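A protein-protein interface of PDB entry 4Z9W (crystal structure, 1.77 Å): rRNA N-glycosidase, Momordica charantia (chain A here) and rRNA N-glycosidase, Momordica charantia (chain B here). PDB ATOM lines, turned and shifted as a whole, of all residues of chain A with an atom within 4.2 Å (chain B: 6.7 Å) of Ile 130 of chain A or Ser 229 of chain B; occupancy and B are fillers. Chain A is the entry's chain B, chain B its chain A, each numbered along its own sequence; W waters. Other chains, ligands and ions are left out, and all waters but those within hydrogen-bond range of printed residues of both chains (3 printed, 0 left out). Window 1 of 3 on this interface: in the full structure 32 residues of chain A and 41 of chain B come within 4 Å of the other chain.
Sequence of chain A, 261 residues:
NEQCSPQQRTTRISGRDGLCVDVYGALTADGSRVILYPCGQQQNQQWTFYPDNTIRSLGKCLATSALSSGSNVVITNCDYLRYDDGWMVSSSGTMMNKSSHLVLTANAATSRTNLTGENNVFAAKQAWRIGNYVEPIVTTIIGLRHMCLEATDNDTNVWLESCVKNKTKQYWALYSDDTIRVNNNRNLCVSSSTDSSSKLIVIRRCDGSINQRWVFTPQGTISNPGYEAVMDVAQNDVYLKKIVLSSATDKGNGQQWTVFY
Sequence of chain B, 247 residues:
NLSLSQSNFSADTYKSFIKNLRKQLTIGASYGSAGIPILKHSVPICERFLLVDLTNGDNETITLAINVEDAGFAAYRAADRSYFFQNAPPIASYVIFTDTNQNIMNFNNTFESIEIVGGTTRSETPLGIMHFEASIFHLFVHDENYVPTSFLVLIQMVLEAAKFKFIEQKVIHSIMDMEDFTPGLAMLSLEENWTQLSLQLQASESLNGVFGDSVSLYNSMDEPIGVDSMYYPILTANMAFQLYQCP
Among the printed residues, merely in contact across the chains: Gly 131 of chain A with Asp 228 of chain B, Val 89 of chain A with Tyr 231 of chain B, Gly 131 of chain A with Tyr 232 of chain B, Arg 129 of chain A with Tyr 231 of chain B, Phe 49 of chain A with Leu 207 of chain B, Ile 130 of chain A with Val 210 of chain B, Ile 130 of chain A with Tyr 231 of chain B, Phe 49 of chain A with Val 210 of chain B and Arg 129 of chain A with Tyr 232 of chain B.
N of Val 89 of chain A is in hydrogen-bond range of OD1 of Asn 208 of chain B (3.0 Å).
The side-chain carboxylate of Asp 228 of chain B is in hydrogen-bond range of the side-chain hydroxyl of Thr 11 of chain A.
OG of Ser 229 of chain B sits at hydrogen-bond distance from O of Ile 130 of chain A (2.6 Å).
Printed residues of chain B within 4 Å of Ile 130 of chain A: Val 210, Ser 229 and Tyr 231.
Ser 229 of chain B touches one residue of chain A.
Of the printed residues of chain A, Val 210 of chain B touches Phe 49 (3.7 Å) and Ile 130 (3.5 Å).
Printed residues of chain A within 4 Å of Leu 207 of chain B: Phe 49 (3.5 Å).
Of the printed residues of chain B, Val 89 of chain A touches Asn 208 and Tyr 231.
Gly 209 of chain B touches none of the printed residues of chain A.
The nearest residue of chain B that does not touch Ile 130 of chain A is Tyr 232 of chain B (4.1 Å).
The nearest printed residue of chain A that does not touch Ser 229 of chain B is Gly 131 of chain A (4.6 Å).
The nearest printed residue of chain B that does not touch Phe 49 of chain A is Asn 208 of chain B (4.3 Å).
Hydrophobic or aromatic side chains of chain A that line the printed part of chain B: Phe 49, Val 89 and Ile 130.
Of the 18 printed residues of chain B, 7 touch a printed residue of chain A.
Hydrophobic or aromatic side chains of chain B within 4 Å of the printed part of chain A: Leu 207, Val 210, Tyr 231 and Tyr 232.
Among the printed residues, no Asp or Glu carboxylate lies within 4 Å of a Lys or Arg side-chain nitrogen of the other chain.
The side-chain hydroxyl (OH) of Tyr 231 of chain B is in hydrogen-bond range of the backbone carbonyl oxygen (O) of Asn 208 of chain B, 2.7 Å away.
The backbone NH (N) of Phe 211 of chain B sits at hydrogen-bond distance from the backbone carbonyl oxygen (O) of Asp 228 of chain B (2.9 Å).
OG of Ser 229 of chain B lies within hydrogen-bond range of N of Tyr 231 of chain B (3.0 Å).
The backbone carbonyl oxygen of Tyr 232 of chain B is in hydrogen-bond range of the side-chain hydroxyl of Thr 236 of chain B.
The backbone carbonyl oxygen (O) of Arg 12 of chain A lies within hydrogen-bond range of the backbone NH (N) of Gly 131 of chain A, at 2.8 Å.
Water W3 lies within hydrogen-bond range of the backbone carbonyl oxygen of Tyr 231 of chain B (2.7 Å) and the guanidinium group of Arg 129 of chain A (2.8 Å).
Water W2 lies within hydrogen-bond range of the backbone carbonyl oxygen (O) of Val 89 of chain A (2.8 Å), the side-chain hydroxyl (OH) of Tyr 231 of chain B (2.9 Å) and the side-chain sulfur (SD) of Met 230 of chain B (3.5 Å).
Water W1 bridges the backbone carbonyl oxygen of Val 89 of chain A (2.8 Å) and the side-chain amide oxygen of Asn 208 of chain B (3.1 Å).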
ATOM      1  N   THR A  11      10.888 -30.178   1.244  1.00  0.00           N
ATOM      2  CA  THR A  11       9.888 -29.655   2.137  1.00  0.00           C
ATOM      3  C   THR A  11       9.124 -30.841   2.779  1.00  0.00           C
ATOM      4  O   THR A  11       9.558 -31.977   2.681  1.00  0.00           O
ATOM      5  CB  THR A  11       8.973 -28.692   1.355  1.00  0.00           C
ATOM      6  OG1 THR A  11       8.115 -27.995   2.251  1.00  0.00           O
ATOM      7  CG2 THR A  11       8.141 -29.418   0.311  1.00  0.00           C
ATOM      8  N   ARG A  12       8.034 -30.551   3.480  1.00  0.00           N
ATOM      9  CA  ARG A  12       7.197 -31.594   4.052  1.00  0.00           C
ATOM     10  C   ARG A  12       5.834 -31.452   3.417  1.00  0.00           C
ATOM     11  O   ARG A  12       5.586 -30.459   2.698  1.00  0.00           O
ATOM     12  CB  ARG A  12       7.162 -31.496   5.560  1.00  0.00           C
ATOM     13  CG  ARG A  12       8.518 -31.813   6.201  1.00  0.00           C
ATOM     14  CD  ARG A  12       8.447 -31.964   7.712  1.00  0.00           C
ATOM     15  NE  ARG A  12       8.184 -30.697   8.406  1.00  0.00           N
ATOM     16  CZ  ARG A  12       7.976 -30.576   9.709  1.00  0.00           C
ATOM     17  NH1 ARG A  12       8.003 -31.649  10.507  1.00  0.00           N
ATOM     18  NH2 ARG A  12       7.760 -29.384  10.244  1.00  0.00           N
ATOM     19  N   PHE A  49      10.758 -31.750  -4.398  1.00  0.00           N
ATOM     20  CA  PHE A  49      10.028 -31.429  -5.608  1.00  0.00           C
ATOM     21  C   PHE A  49      11.047 -30.993  -6.649  1.00  0.00           C
ATOM     22  O   PHE A  49      11.993 -30.250  -6.326  1.00  0.00           O
ATOM     23  CB  PHE A  49       9.025 -30.304  -5.360  1.00  0.00           C
ATOM     24  CG  PHE A  49       7.849 -30.729  -4.536  1.00  0.00           C
ATOM     25  CD1 PHE A  49       8.006 -30.995  -3.185  1.00  0.00           C
ATOM     26  CD2 PHE A  49       6.617 -30.895  -5.110  1.00  0.00           C
ATOM     27  CE1 PHE A  49       6.924 -31.393  -2.420  1.00  0.00           C
ATOM     28  CE2 PHE A  49       5.529 -31.320  -4.356  1.00  0.00           C
ATOM     29  CZ  PHE A  49       5.691 -31.558  -3.026  1.00  0.00           C
ATOM     30  N   VAL A  89      -0.273 -30.475  -8.748  1.00  0.00           N
ATOM     31  CA  VAL A  89      -0.836 -29.987  -7.513  1.00  0.00           C
ATOM     32  C   VAL A  89      -1.635 -28.742  -7.855  1.00  0.00           C
ATOM     33  O   VAL A  89      -1.107 -27.813  -8.451  1.00  0.00           O
ATOM     34  CB  VAL A  89       0.231 -29.633  -6.472  1.00  0.00           C
ATOM     35  CG1 VAL A  89      -0.436 -29.215  -5.165  1.00  0.00           C
ATOM     36  CG2 VAL A  89       1.168 -30.817  -6.252  1.00  0.00           C
ATOM     37  N   TRP A 128      -4.136 -30.909   0.941  1.00  0.00           N
ATOM     38  CA  TRP A 128      -2.776 -30.997   1.395  1.00  0.00           C
ATOM     39  C   TRP A 128      -2.151 -29.622   1.410  1.00  0.00           C
ATOM     40  O   TRP A 128      -2.490 -28.787   0.556  1.00  0.00           O
ATOM     41  CB  TRP A 128      -1.988 -31.902   0.450  1.00  0.00           C
ATOM     42  CG  TRP A 128      -2.623 -33.266   0.384  1.00  0.00           C
ATOM     43  CD1 TRP A 128      -3.504 -33.731  -0.561  1.00  0.00           C
ATOM     44  CD2 TRP A 128      -2.516 -34.278   1.367  1.00  0.00           C
ATOM     45  NE1 TRP A 128      -3.912 -35.003  -0.239  1.00  0.00           N
ATOM     46  CE2 TRP A 128      -3.311 -35.368   0.940  1.00  0.00           C
ATOM     47  CE3 TRP A 128      -1.785 -34.398   2.550  1.00  0.00           C
ATOM     48  CZ2 TRP A 128      -3.422 -36.544   1.678  1.00  0.00           C
ATOM     49  CZ3 TRP A 128      -1.906 -35.575   3.300  1.00  0.00           C
ATOM     50  CH2 TRP A 128      -2.694 -36.640   2.840  1.00  0.00           C
ATOM     51  N   ARG A 129      -1.311 -29.377   2.409  1.00  0.00           N
ATOM     52  CA  ARG A 129      -0.393 -28.240   2.428  1.00  0.00           C
ATOM     53  C   ARG A 129       1.007 -28.752   2.223  1.00  0.00           C
ATOM     54  O   ARG A 129       1.575 -29.392   3.092  1.00  0.00           O
ATOM     55  CB  ARG A 129      -0.453 -27.499   3.733  1.00  0.00           C
ATOM     56  CG  ARG A 129       0.498 -26.328   3.814  1.00  0.00           C
ATOM     57  CD  ARG A 129       0.763 -25.925   5.225  1.00  0.00           C
ATOM     58  NE  ARG A 129      -0.432 -25.449   5.903  1.00  0.00           N
ATOM     59  CZ  ARG A 129      -0.473 -25.192   7.201  1.00  0.00           C
ATOM     60  NH1 ARG A 129       0.616 -25.330   7.960  1.00  0.00           N
ATOM     61  NH2 ARG A 129      -1.600 -24.783   7.763  1.00  0.00           N
ATOM     62  N   ILE A 130       1.576 -28.443   1.074  1.00  0.00           N
ATOM     63  CA  ILE A 130       2.977 -28.742   0.824  1.00  0.00           C
ATOM     64  C   ILE A 130       3.731 -27.555   1.438  1.00  0.00           C
ATOM     65  O   ILE A 130       3.484 -26.413   1.089  1.00  0.00           O
ATOM     66  CB  ILE A 130       3.282 -28.866  -0.674  1.00  0.00           C
ATOM     67  CG1 ILE A 130       2.494 -30.020  -1.297  1.00  0.00           C
ATOM     68  CG2 ILE A 130       4.787 -28.989  -0.907  1.00  0.00           C
ATOM     69  CD1 ILE A 130       2.412 -29.894  -2.798  1.00  0.00           C
ATOM     70  N   GLY A 131       4.610 -27.847   2.380  1.00  0.00           N
ATOM     71  CA  GLY A 131       5.355 -26.827   3.073  1.00  0.00           C
ATOM     72  C   GLY A 131       6.015 -27.301   4.335  1.00  0.00           C
ATOM     73  O   GLY A 131       5.547 -28.243   4.980  1.00  0.00           O
ATOM     74  N   LEU B 201       6.452 -16.881  -5.923  1.00  0.00           N
ATOM     75  CA  LEU B 201       5.193 -17.307  -6.475  1.00  0.00           C
ATOM     76  C   LEU B 201       5.309 -17.587  -7.962  1.00  0.00           C
ATOM     77  O   LEU B 201       4.819 -18.630  -8.460  1.00  0.00           O
ATOM     78  CB  LEU B 201       4.118 -16.240  -6.238  1.00  0.00           C
ATOM     79  CG  LEU B 201       3.506 -16.199  -4.848  1.00  0.00           C
ATOM     80  CD1 LEU B 201       2.754 -14.895  -4.678  1.00  0.00           C
ATOM     81  CD2 LEU B 201       2.595 -17.419  -4.650  1.00  0.00           C
ATOM     82  N   SER B 204       7.600 -20.570  -8.716  1.00  0.00           N
ATOM     83  CA  SER B 204       6.971 -21.810  -8.273  1.00  0.00           C
ATOM     84  C   SER B 204       6.113 -22.527  -9.307  1.00  0.00           C
ATOM     85  O   SER B 204       5.757 -23.692  -9.108  1.00  0.00           O
ATOM     86  CB  SER B 204       6.132 -21.552  -7.033  1.00  0.00           C
ATOM     87  OG  SER B 204       4.882 -20.995  -7.379  1.00  0.00           O
ATOM     88  N   LEU B 207       7.600 -25.759 -10.153  1.00  0.00           N
ATOM     89  CA  LEU B 207       7.821 -26.713  -9.055  1.00  0.00           C
ATOM     90  C   LEU B 207       6.527 -27.062  -8.332  1.00  0.00           C
ATOM     91  O   LEU B 207       6.535 -27.243  -7.128  1.00  0.00           O
ATOM     92  CB  LEU B 207       8.798 -26.167  -8.017  1.00  0.00           C
ATOM     93  CG  LEU B 207      10.289 -26.458  -8.042  1.00  0.00           C
ATOM     94  CD1 LEU B 207      10.907 -26.177  -6.674  1.00  0.00           C
ATOM     95  CD2 LEU B 207      10.585 -27.858  -8.531  1.00  0.00           C
ATOM     96  N   ASN B 208       5.425 -27.173  -9.060  1.00  0.00           N
ATOM     97  CA  ASN B 208       4.124 -27.551  -8.477  1.00  0.00           C
ATOM     98  C   ASN B 208       3.696 -26.642  -7.307  1.00  0.00           C
ATOM     99  O   ASN B 208       3.086 -27.089  -6.328  1.00  0.00           O
ATOM    100  CB  ASN B 208       4.151 -29.040  -8.047  1.00  0.00           C
ATOM    101  CG  ASN B 208       3.539 -29.968  -9.068  1.00  0.00           C
ATOM    102  OD1 ASN B 208       2.470 -29.716  -9.616  1.00  0.00           O
ATOM    103  ND2 ASN B 208       4.193 -31.106  -9.277  1.00  0.00           N
ATOM    104  N   GLY B 209       4.055 -25.363  -7.407  1.00  0.00           N
ATOM    105  CA  GLY B 209       3.683 -24.375  -6.402  1.00  0.00           C
ATOM    106  C   GLY B 209       4.622 -24.271  -5.220  1.00  0.00           C
ATOM    107  O   GLY B 209       4.343 -23.518  -4.289  1.00  0.00           O
ATOM    108  N   VAL B 210       5.725 -25.002  -5.254  1.00  0.00           N
ATOM    109  CA  VAL B 210       6.702 -24.981  -4.184  1.00  0.00           C
ATOM    110  C   VAL B 210       7.728 -23.916  -4.544  1.00  0.00           C
ATOM    111  O   VAL B 210       8.116 -23.795  -5.713  1.00  0.00           O
ATOM    112  CB  VAL B 210       7.379 -26.355  -3.999  1.00  0.00           C
ATOM    113  CG1 VAL B 210       8.427 -26.302  -2.891  1.00  0.00           C
ATOM    114  CG2 VAL B 210       6.322 -27.416  -3.692  1.00  0.00           C
ATOM    115  N   PHE B 211       8.126 -23.146  -3.549  1.00  0.00           N
ATOM    116  CA  PHE B 211       9.101 -22.063  -3.709  1.00  0.00           C
ATOM    117  C   PHE B 211      10.546 -22.553  -3.802  1.00  0.00           C
ATOM    118  O   PHE B 211      10.917 -23.589  -3.269  1.00  0.00           O
ATOM    119  CB  PHE B 211       9.041 -21.099  -2.545  1.00  0.00           C
ATOM    120  CG  PHE B 211       7.780 -20.263  -2.450  1.00  0.00           C
ATOM    121  CD1 PHE B 211       6.702 -20.399  -3.335  1.00  0.00           C
ATOM    122  CD2 PHE B 211       7.699 -19.321  -1.439  1.00  0.00           C
ATOM    123  CE1 PHE B 211       5.571 -19.587  -3.201  1.00  0.00           C
ATOM    124  CE2 PHE B 211       6.565 -18.514  -1.306  1.00  0.00           C
ATOM    125  CZ  PHE B 211       5.517 -18.650  -2.193  1.00  0.00           C
ATOM    126  N   ASP B 213      12.956 -20.684  -2.338  1.00  0.00           N
ATOM    127  CA  ASP B 213      13.471 -20.279  -1.046  1.00  0.00           C
ATOM    128  C   ASP B 213      12.285 -19.973  -0.168  1.00  0.00           C
ATOM    129  O   ASP B 213      11.261 -19.449  -0.654  1.00  0.00           O
ATOM    130  CB  ASP B 213      14.339 -19.021  -1.163  1.00  0.00           C
ATOM    131  CG  ASP B 213      15.739 -19.318  -1.703  1.00  0.00           C
ATOM    132  OD1 ASP B 213      16.487 -20.127  -1.082  1.00  0.00           O
ATOM    133  OD2 ASP B 213      16.093 -18.734  -2.754  1.00  0.00           O
ATOM    134  N   SER B 214      12.413 -20.275   1.113  1.00  0.00           N
ATOM    135  CA  SER B 214      11.375 -19.917   2.096  1.00  0.00           C
ATOM    136  C   SER B 214      11.406 -18.429   2.454  1.00  0.00           C
ATOM    137  O   SER B 214      12.472 -17.783   2.459  1.00  0.00           O
ATOM    138  CB  SER B 214      11.576 -20.764   3.349  1.00  0.00           C
ATOM    139  OG  SER B 214      10.499 -20.581   4.246  1.00  0.00           O
ATOM    140  N   GLY B 226       7.199 -19.890   8.223  1.00  0.00           N
ATOM    141  CA  GLY B 226       7.920 -20.136   6.976  1.00  0.00           C
ATOM    142  C   GLY B 226       6.943 -20.354   5.845  1.00  0.00           C
ATOM    143  O   GLY B 226       6.125 -21.262   5.896  1.00  0.00           O
ATOM    144  N   VAL B 227       6.998 -19.494   4.824  1.00  0.00           N
ATOM    145  CA  VAL B 227       6.219 -19.705   3.626  1.00  0.00           C
ATOM    146  C   VAL B 227       7.157 -20.147   2.515  1.00  0.00           C
ATOM    147  O   VAL B 227       7.925 -19.333   1.953  1.00  0.00           O
ATOM    148  CB  VAL B 227       5.424 -18.457   3.230  1.00  0.00           C
ATOM    149  CG1 VAL B 227       4.588 -18.733   1.979  1.00  0.00           C
ATOM    150  CG2 VAL B 227       4.558 -18.002   4.394  1.00  0.00           C
ATOM    151  N   ASP B 228       7.104 -21.432   2.198  1.00  0.00           N
ATOM    152  CA  ASP B 228       7.953 -22.043   1.165  1.00  0.00           C
ATOM    153  C   ASP B 228       7.103 -22.648   0.056  1.00  0.00           C
ATOM    154  O   ASP B 228       7.579 -23.461  -0.730  1.00  0.00           O
ATOM    155  CB  ASP B 228       8.944 -23.057   1.761  1.00  0.00           C
ATOM    156  CG  ASP B 228       8.237 -24.290   2.358  1.00  0.00           C
ATOM    157  OD1 ASP B 228       7.055 -24.145   2.702  1.00  0.00           O
ATOM    158  OD2 ASP B 228       8.863 -25.368   2.488  1.00  0.00           O
ATOM    159  N   SER B 229       5.864 -22.193  -0.073  1.00  0.00           N
ATOM    160  CA  SER B 229       5.001 -22.614  -1.145  1.00  0.00           C
ATOM    161  C   SER B 229       3.828 -21.678  -1.255  1.00  0.00           C
ATOM    162  O   SER B 229       3.612 -20.817  -0.397  1.00  0.00           O
ATOM    163  CB  SER B 229       4.476 -24.025  -0.853  1.00  0.00           C
ATOM    164  OG  SER B 229       3.441 -23.963   0.098  1.00  0.00           O
ATOM    165  N   MET B 230       3.038 -21.853  -2.296  1.00  0.00           N
ATOM    166  CA  MET B 230       1.835 -21.036  -2.442  1.00  0.00           C
ATOM    167  C   MET B 230       0.675 -21.503  -1.540  1.00  0.00           C
ATOM    168  O   MET B 230      -0.398 -20.907  -1.586  1.00  0.00           O
ATOM    169  CB  MET B 230       1.369 -21.059  -3.902  1.00  0.00           C
ATOM    170  CG  MET B 230       0.877 -22.420  -4.401  1.00  0.00           C
ATOM    171  SD  MET B 230       0.068 -22.275  -6.002  1.00  0.00           S
ATOM    172  CE  MET B 230      -1.413 -21.511  -5.427  1.00  0.00           C
ATOM    173  N   TYR B 231       0.881 -22.551  -0.740  1.00  0.00           N
ATOM    174  CA  TYR B 231      -0.225 -23.223  -0.010  1.00  0.00           C
ATOM    175  C   TYR B 231      -0.377 -22.719   1.429  1.00  0.00           C
ATOM    176  O   TYR B 231      -0.709 -23.500   2.341  1.00  0.00           O
ATOM    177  CB  TYR B 231       0.001 -24.737  -0.058  1.00  0.00           C
ATOM    178  CG  TYR B 231       0.208 -25.176  -1.467  1.00  0.00           C
ATOM    179  CD1 TYR B 231      -0.827 -25.109  -2.373  1.00  0.00           C
ATOM    180  CD2 TYR B 231       1.441 -25.585  -1.927  1.00  0.00           C
ATOM    181  CE1 TYR B 231      -0.661 -25.467  -3.679  1.00  0.00           C
ATOM    182  CE2 TYR B 231       1.622 -25.966  -3.247  1.00  0.00           C
ATOM    183  CZ  TYR B 231       0.569 -25.891  -4.121  1.00  0.00           C
ATOM    184  OH  TYR B 231       0.685 -26.229  -5.440  1.00  0.00           O
ATOM    185  N   TYR B 232      -0.163 -21.417   1.624  1.00  0.00           N
ATOM    186  CA  TYR B 232      -0.299 -20.739   2.910  1.00  0.00           C
ATOM    187  C   TYR B 232      -1.339 -19.639   2.785  1.00  0.00           C
ATOM    188  O   TYR B 232      -1.119 -18.681   2.036  1.00  0.00           O
ATOM    189  CB  TYR B 232       1.040 -20.166   3.389  1.00  0.00           C
ATOM    190  CG  TYR B 232       1.952 -21.264   3.866  1.00  0.00           C
ATOM    191  CD1 TYR B 232       2.773 -21.938   2.972  1.00  0.00           C
ATOM    192  CD2 TYR B 232       1.928 -21.686   5.178  1.00  0.00           C
ATOM    193  CE1 TYR B 232       3.573 -22.992   3.386  1.00  0.00           C
ATOM    194  CE2 TYR B 232       2.732 -22.729   5.614  1.00  0.00           C
ATOM    195  CZ  TYR B 232       3.553 -23.370   4.717  1.00  0.00           C
ATOM    196  OH  TYR B 232       4.329 -24.422   5.115  1.00  0.00           O
ATOM    197  N   LEU B 235      -0.507 -15.917   2.885  1.00  0.00           N
ATOM    198  CA  LEU B 235      -0.014 -15.317   1.659  1.00  0.00           C
ATOM    199  C   LEU B 235      -1.170 -15.151   0.686  1.00  0.00           C
ATOM    200  O   LEU B 235      -1.419 -14.064   0.193  1.00  0.00           O
ATOM    201  CB  LEU B 235       1.103 -16.183   1.038  1.00  0.00           C
ATOM    202  CG  LEU B 235       1.592 -15.739  -0.339  1.00  0.00           C
ATOM    203  CD1 LEU B 235       2.105 -14.322  -0.228  1.00  0.00           C
ATOM    204  CD2 LEU B 235       2.674 -16.667  -0.903  1.00  0.00           C
ATOM    205  N   THR B 236      -1.892 -16.236   0.404  1.00  0.00           N
ATOM    206  CA  THR B 236      -2.850 -16.219  -0.687  1.00  0.00           C
ATOM    207  C   THR B 236      -4.177 -15.522  -0.383  1.00  0.00           C
ATOM    208  O   THR B 236      -4.836 -15.034  -1.302  1.00  0.00           O
ATOM    209  CB  THR B 236      -3.019 -17.630  -1.287  1.00  0.00           C
ATOM    210  OG1 THR B 236      -3.441 -18.517  -0.280  1.00  0.00           O
ATOM    211  CG2 THR B 236      -1.690 -18.126  -1.825  1.00  0.00           C
HETATM  212  O   HOH W   1       0.621 -27.476 -10.692  1.00  0.00           O
HETATM  213  O   HOH W   2      -0.313 -25.144  -7.891  1.00  0.00           O
HETATM  214  O   HOH W   3      -2.436 -24.619   4.068  1.00  0.00           O
